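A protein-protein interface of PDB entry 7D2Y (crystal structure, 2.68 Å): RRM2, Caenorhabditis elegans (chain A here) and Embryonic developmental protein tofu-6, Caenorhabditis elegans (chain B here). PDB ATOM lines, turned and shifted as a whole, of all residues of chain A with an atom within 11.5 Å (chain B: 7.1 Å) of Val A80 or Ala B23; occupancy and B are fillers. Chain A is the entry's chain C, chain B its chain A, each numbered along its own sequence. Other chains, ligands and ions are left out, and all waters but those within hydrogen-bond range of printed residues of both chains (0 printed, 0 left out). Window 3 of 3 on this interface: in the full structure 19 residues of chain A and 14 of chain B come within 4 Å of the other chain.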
ATOM      1  N   SER A  76       0.630  -0.691  27.496  1.00  0.00           N
ATOM      2  CA  SER A  76       1.397  -1.680  26.748  1.00  0.00           C
ATOM      3  C   SER A  76       0.450  -2.613  25.998  1.00  0.00           C
ATOM      4  O   SER A  76      -0.440  -3.218  26.600  1.00  0.00           O
ATOM      5  CB  SER A  76       2.281  -2.461  27.711  1.00  0.00           C
ATOM      6  OG  SER A  76       2.792  -3.640  27.109  1.00  0.00           O
ATOM      7  N   SER A  77       0.616  -2.730  24.683  1.00  0.00           N
ATOM      8  CA  SER A  77      -0.349  -3.442  23.839  1.00  0.00           C
ATOM      9  C   SER A  77       0.347  -4.388  22.870  1.00  0.00           C
ATOM     10  O   SER A  77       0.385  -4.150  21.654  1.00  0.00           O
ATOM     11  CB  SER A  77      -1.228  -2.443  23.092  1.00  0.00           C
ATOM     12  OG  SER A  77      -1.851  -1.594  24.043  1.00  0.00           O
ATOM     13  N   PRO A  78       0.891  -5.490  23.371  1.00  0.00           N
ATOM     14  CA  PRO A  78       1.550  -6.442  22.470  1.00  0.00           C
ATOM     15  C   PRO A  78       0.530  -7.060  21.532  1.00  0.00           C
ATOM     16  O   PRO A  78      -0.634  -7.247  21.888  1.00  0.00           O
ATOM     17  CB  PRO A  78       2.153  -7.479  23.418  1.00  0.00           C
ATOM     18  CG  PRO A  78       1.300  -7.388  24.655  1.00  0.00           C
ATOM     19  CD  PRO A  78       0.801  -5.980  24.757  1.00  0.00           C
ATOM     20  N   ALA A  79       0.958  -7.325  20.302  1.00  0.00           N
ATOM     21  CA  ALA A  79       0.035  -7.945  19.364  1.00  0.00           C
ATOM     22  C   ALA A  79      -0.207  -9.406  19.741  1.00  0.00           C
ATOM     23  O   ALA A  79      -1.359  -9.858  19.793  1.00  0.00           O
ATOM     24  CB  ALA A  79       0.559  -7.792  17.936  1.00  0.00           C
ATOM     25  N   VAL A  80       0.859 -10.147  20.042  1.00  0.00           N
ATOM     26  CA  VAL A  80       0.743 -11.496  20.590  1.00  0.00           C
ATOM     27  C   VAL A  80       1.195 -11.464  22.043  1.00  0.00           C
ATOM     28  O   VAL A  80       2.070 -10.666  22.402  1.00  0.00           O
ATOM     29  CB  VAL A  80       1.558 -12.517  19.778  1.00  0.00           C
ATOM     30  CG1 VAL A  80       1.533 -12.166  18.316  1.00  0.00           C
ATOM     31  CG2 VAL A  80       2.989 -12.627  20.283  1.00  0.00           C
ATOM     32  N   PRO A  81       0.621 -12.290  22.911  1.00  0.00           N
ATOM     33  CA  PRO A  81       1.063 -12.324  24.309  1.00  0.00           C
ATOM     34  C   PRO A  81       2.561 -12.543  24.452  1.00  0.00           C
ATOM     35  O   PRO A  81       3.210 -13.161  23.606  1.00  0.00           O
ATOM     36  CB  PRO A  81       0.269 -13.496  24.895  1.00  0.00           C
ATOM     37  CG  PRO A  81      -1.014 -13.469  24.111  1.00  0.00           C
ATOM     38  CD  PRO A  81      -0.639 -13.031  22.709  1.00  0.00           C
ATOM     39  N   LEU A  82       3.100 -12.018  25.545  1.00  0.00           N
ATOM     40  CA  LEU A  82       4.527 -12.090  25.836  1.00  0.00           C
ATOM     41  C   LEU A  82       4.899 -13.411  26.494  1.00  0.00           C
ATOM     42  O   LEU A  82       6.069 -13.656  26.789  1.00  0.00           O
ATOM     43  CB  LEU A  82       4.930 -10.917  26.733  1.00  0.00           C
ATOM     44  CG  LEU A  82       4.545  -9.530  26.201  1.00  0.00           C
ATOM     45  CD1 LEU A  82       4.672  -8.467  27.278  1.00  0.00           C
ATOM     46  CD2 LEU A  82       5.408  -9.155  25.005  1.00  0.00           C
ATOM     47  N   ILE B  20      12.053 -10.897  12.600  1.00  0.00           N
ATOM     48  CA  ILE B  20      11.036 -10.738  13.646  1.00  0.00           C
ATOM     49  C   ILE B  20       9.789 -11.526  13.248  1.00  0.00           C
ATOM     50  O   ILE B  20       9.317 -11.378  12.108  1.00  0.00           O
ATOM     51  CB  ILE B  20      10.699  -9.256  13.841  1.00  0.00           C
ATOM     52  CG1 ILE B  20      11.900  -8.460  14.362  1.00  0.00           C
ATOM     53  CG2 ILE B  20       9.478  -9.085  14.755  1.00  0.00           C
ATOM     54  CD1 ILE B  20      11.729  -6.964  14.252  1.00  0.00           C
ATOM     55  N   PRO B  21       9.215 -12.332  14.140  1.00  0.00           N
ATOM     56  CA  PRO B  21       7.962 -13.028  13.814  1.00  0.00           C
ATOM     57  C   PRO B  21       6.916 -12.079  13.244  1.00  0.00           C
ATOM     58  O   PRO B  21       6.818 -10.916  13.639  1.00  0.00           O
ATOM     59  CB  PRO B  21       7.518 -13.605  15.160  1.00  0.00           C
ATOM     60  CG  PRO B  21       8.770 -13.750  15.929  1.00  0.00           C
ATOM     61  CD  PRO B  21       9.674 -12.628  15.505  1.00  0.00           C
ATOM     62  N   LYS B  22       6.122 -12.591  12.308  1.00  0.00           N
ATOM     63  CA  LYS B  22       5.239 -11.738  11.528  1.00  0.00           C
ATOM     64  C   LYS B  22       4.109 -11.140  12.360  1.00  0.00           C
ATOM     65  O   LYS B  22       3.526 -10.122  11.961  1.00  0.00           O
ATOM     66  CB  LYS B  22       4.663 -12.532  10.354  1.00  0.00           C
ATOM     67  CG  LYS B  22       3.676 -13.628  10.753  1.00  0.00           C
ATOM     68  N   ALA B  23       3.792 -11.732  13.503  1.00  0.00           N
ATOM     69  CA  ALA B  23       2.644 -11.289  14.285  1.00  0.00           C
ATOM     70  C   ALA B  23       2.986 -10.197  15.299  1.00  0.00           C
ATOM     71  O   ALA B  23       2.073  -9.550  15.827  1.00  0.00           O
ATOM     72  CB  ALA B  23       2.025 -12.488  15.006  1.00  0.00           C
ATOM     73  N   TRP B  24       4.268  -9.987  15.586  1.00  0.00           N
ATOM     74  CA  TRP B  24       4.664  -8.948  16.519  1.00  0.00           C
ATOM     75  C   TRP B  24       4.293  -7.577  15.986  1.00  0.00           C
ATOM     76  O   TRP B  24       4.311  -7.334  14.778  1.00  0.00           O
ATOM     77  CB  TRP B  24       6.167  -8.981  16.756  1.00  0.00           C
ATOM     78  CG  TRP B  24       6.637 -10.171  17.495  1.00  0.00           C
ATOM     79  CD1 TRP B  24       5.959 -11.351  17.708  1.00  0.00           C
ATOM     80  CD2 TRP B  24       7.915 -10.323  18.125  1.00  0.00           C
ATOM     81  NE1 TRP B  24       6.743 -12.218  18.438  1.00  0.00           N
ATOM     82  CE2 TRP B  24       7.946 -11.614  18.703  1.00  0.00           C
ATOM     83  CE3 TRP B  24       9.033  -9.496  18.253  1.00  0.00           C
ATOM     84  CZ2 TRP B  24       9.044 -12.083  19.404  1.00  0.00           C
ATOM     85  CZ3 TRP B  24      10.126  -9.971  18.937  1.00  0.00           C
ATOM     86  CH2 TRP B  24      10.125 -11.255  19.506  1.00  0.00           C
ATOM     87  N   ASN B  25       3.955  -6.674  16.917  1.00  0.00           N
ATOM     88  CA  ASN B  25       3.979  -5.234  16.707  1.00  0.00           C
ATOM     89  C   ASN B  25       5.148  -4.637  17.491  1.00  0.00           C
ATOM     90  O   ASN B  25       5.969  -5.348  18.090  1.00  0.00           O
ATOM     91  CB  ASN B  25       2.644  -4.581  17.098  1.00  0.00           C
ATOM     92  CG  ASN B  25       2.312  -4.734  18.581  1.00  0.00           C
ATOM     93  OD1 ASN B  25       3.031  -5.402  19.340  1.00  0.00           O
ATOM     94  ND2 ASN B  25       1.212  -4.114  19.002  1.00  0.00           N
ATOM     95  N   TRP B  27       5.164  -3.193  20.279  1.00  0.00           N
ATOM     96  CA  TRP B  27       5.189  -3.463  21.711  1.00  0.00           C
ATOM     97  C   TRP B  27       5.936  -4.748  22.006  1.00  0.00           C
ATOM     98  O   TRP B  27       6.750  -4.790  22.937  1.00  0.00           O
ATOM     99  CB  TRP B  27       3.778  -3.514  22.284  1.00  0.00           C
ATOM    100  CG  TRP B  27       3.268  -2.154  22.617  1.00  0.00           C
ATOM    101  CD1 TRP B  27       2.364  -1.429  21.907  1.00  0.00           C
ATOM    102  CD2 TRP B  27       3.659  -1.334  23.730  1.00  0.00           C
ATOM    103  NE1 TRP B  27       2.156  -0.214  22.513  1.00  0.00           N
ATOM    104  CE2 TRP B  27       2.942  -0.131  23.633  1.00  0.00           C
ATOM    105  CE3 TRP B  27       4.553  -1.502  24.797  1.00  0.00           C
ATOM    106  CZ2 TRP B  27       3.083   0.903  24.568  1.00  0.00           C
ATOM    107  CZ3 TRP B  27       4.695  -0.483  25.718  1.00  0.00           C
ATOM    108  CH2 TRP B  27       3.964   0.702  25.604  1.00  0.00           C
ATOM    109  N   ASN B  28       5.671  -5.803  21.223  1.00  0.00           N
ATOM    110  CA  ASN B  28       6.413  -7.049  21.348  1.00  0.00           C
ATOM    111  C   ASN B  28       7.906  -6.791  21.270  1.00  0.00           C
ATOM    112  O   ASN B  28       8.660  -7.143  22.182  1.00  0.00           O
ATOM    113  CB  ASN B  28       6.001  -8.025  20.242  1.00  0.00           C
ATOM    114  CG  ASN B  28       4.717  -8.745  20.544  1.00  0.00           C
ATOM    115  OD1 ASN B  28       3.727  -8.614  19.816  1.00  0.00           O
ATOM    116  ND2 ASN B  28       4.718  -9.514  21.628  1.00  0.00           N
ATOM    117  N   GLY B  51       6.465 -11.287   3.353  1.00  0.00           N
ATOM    118  CA  GLY B  51       5.713 -10.814   4.498  1.00  0.00           C
ATOM    119  C   GLY B  51       5.788 -11.690   5.733  1.00  0.00           C
ATOM    120  O   GLY B  51       5.056 -11.430   6.699  1.00  0.00           O
ATOM    121  N   GLN B  52       6.677 -12.697   5.745  1.00  0.00           N
ATOM    122  CA  GLN B  52       6.753 -13.715   6.792  1.00  0.00           C
ATOM    123  C   GLN B  52       7.567 -13.291   8.011  1.00  0.00           C
ATOM    124  O   GLN B  52       7.329 -13.817   9.108  1.00  0.00           O
ATOM    125  CB  GLN B  52       7.349 -15.012   6.225  1.00  0.00           C
ATOM    126  CG  GLN B  52       6.543 -15.649   5.091  1.00  0.00           C
ATOM    127  CD  GLN B  52       5.090 -15.906   5.455  1.00  0.00           C
ATOM    128  OE1 GLN B  52       4.792 -16.576   6.442  1.00  0.00           O
ATOM    129  NE2 GLN B  52       4.179 -15.376   4.650  1.00  0.00           N
ATOM    130  N   GLN B  54       9.580  -9.571   9.806  1.00  0.00           N
ATOM    131  CA  GLN B  54       9.666  -8.122   9.749  1.00  0.00           C
ATOM    132  C   GLN B  54      11.068  -7.666  10.133  1.00  0.00           C
ATOM    133  O   GLN B  54      11.815  -8.384  10.798  1.00  0.00           O
ATOM    134  CB  GLN B  54       8.634  -7.479  10.676  1.00  0.00           C
ATOM    135  CG  GLN B  54       7.380  -8.279  10.822  1.00  0.00           C
ATOM    136  CD  GLN B  54       6.386  -7.626  11.755  1.00  0.00           C
ATOM    137  OE1 GLN B  54       5.854  -6.543  11.470  1.00  0.00           O
ATOM    138  NE2 GLN B  54       6.128  -8.277  12.885  1.00  0.00           N
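The side-chain amide nitrogen of Asn B25 is in hydrogen-bond range of the backbone carbonyl oxygen of Ser A77. O of Val A80 lies within hydrogen-bond range of ND2 of Asn B28 (3.0 Å). OD1 of Asn B25 is in hydrogen-bond range of N of Ala A79 (3.0 Å). The side-chain amide oxygen (OD1) of Asn B28 lies within hydrogen-bond range of the backbone NH (N) of Ala A79.
The backbone NH (N) of Trp B27 lies close to the side-chain amide oxygen (OD1) of Asn B25, at 3.2 Å. N of Asn B28 sits at hydrogen-bond distance from OD1 of Asn B25 (3.3 Å).
Ser A76 touches Trp B27. Ser A77 touches Trp B27 (O to CD1, 3.4 Å). OD1 of Asn B25 touches CA of Pro A78 (3.6 Å). Pro A78 touches Trp B27 (N to CB, 3.7 Å). CB of Pro A78 touches ND2 of Asn B28, 3.7 Å away. CB of Ala A79 touches O of Ala B23, 3.1 Å away. Ala B23 touches Val A80 (CB to CG1, 3.4 Å). Asn B28 touches Leu A82 (ND2 to CD2, 3.5 Å).
Val A80 touches just these residues of chain B: Ala B23 (3.4 Å) and Asn B28 (3.0 Å). Ala B23 touches just these residues of chain A: Ala A79 (3.1 Å) and Val A80 (3.4 Å). No residue of chain A comes within 4 Å of Pro B21. No residue of chain A comes within 4 Å of Lys B22. Of the printed residues of chain B, Pro A78 touches Asn B25, Trp B27 and Asn B28. Printed residues of chain B within 4 Å of Leu A82: Asn B28. The nearest residue of chain A that does not touch Ala B23 is Pro A78 (6.4 Å). The nearest printed residue of chain B that does not touch Ala A79 is Trp B24 (4.2 Å).
Hydrophobic or aromatic side chains of chain A within 4 Å of the printed part of chain B: Pro A78, Ala A79, Val A80 and Leu A82. Of the 11 printed residues of chain B, 4 touch a printed residue of chain A. Hydrophobic or aromatic side chains of chain B that line the printed part of chain A: Ala B23 and Trp B27. Among the printed residues, no Asp or Glu carboxylate lies within 4 Å of a Lys or Arg side-chain nitrogen of the other chain.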
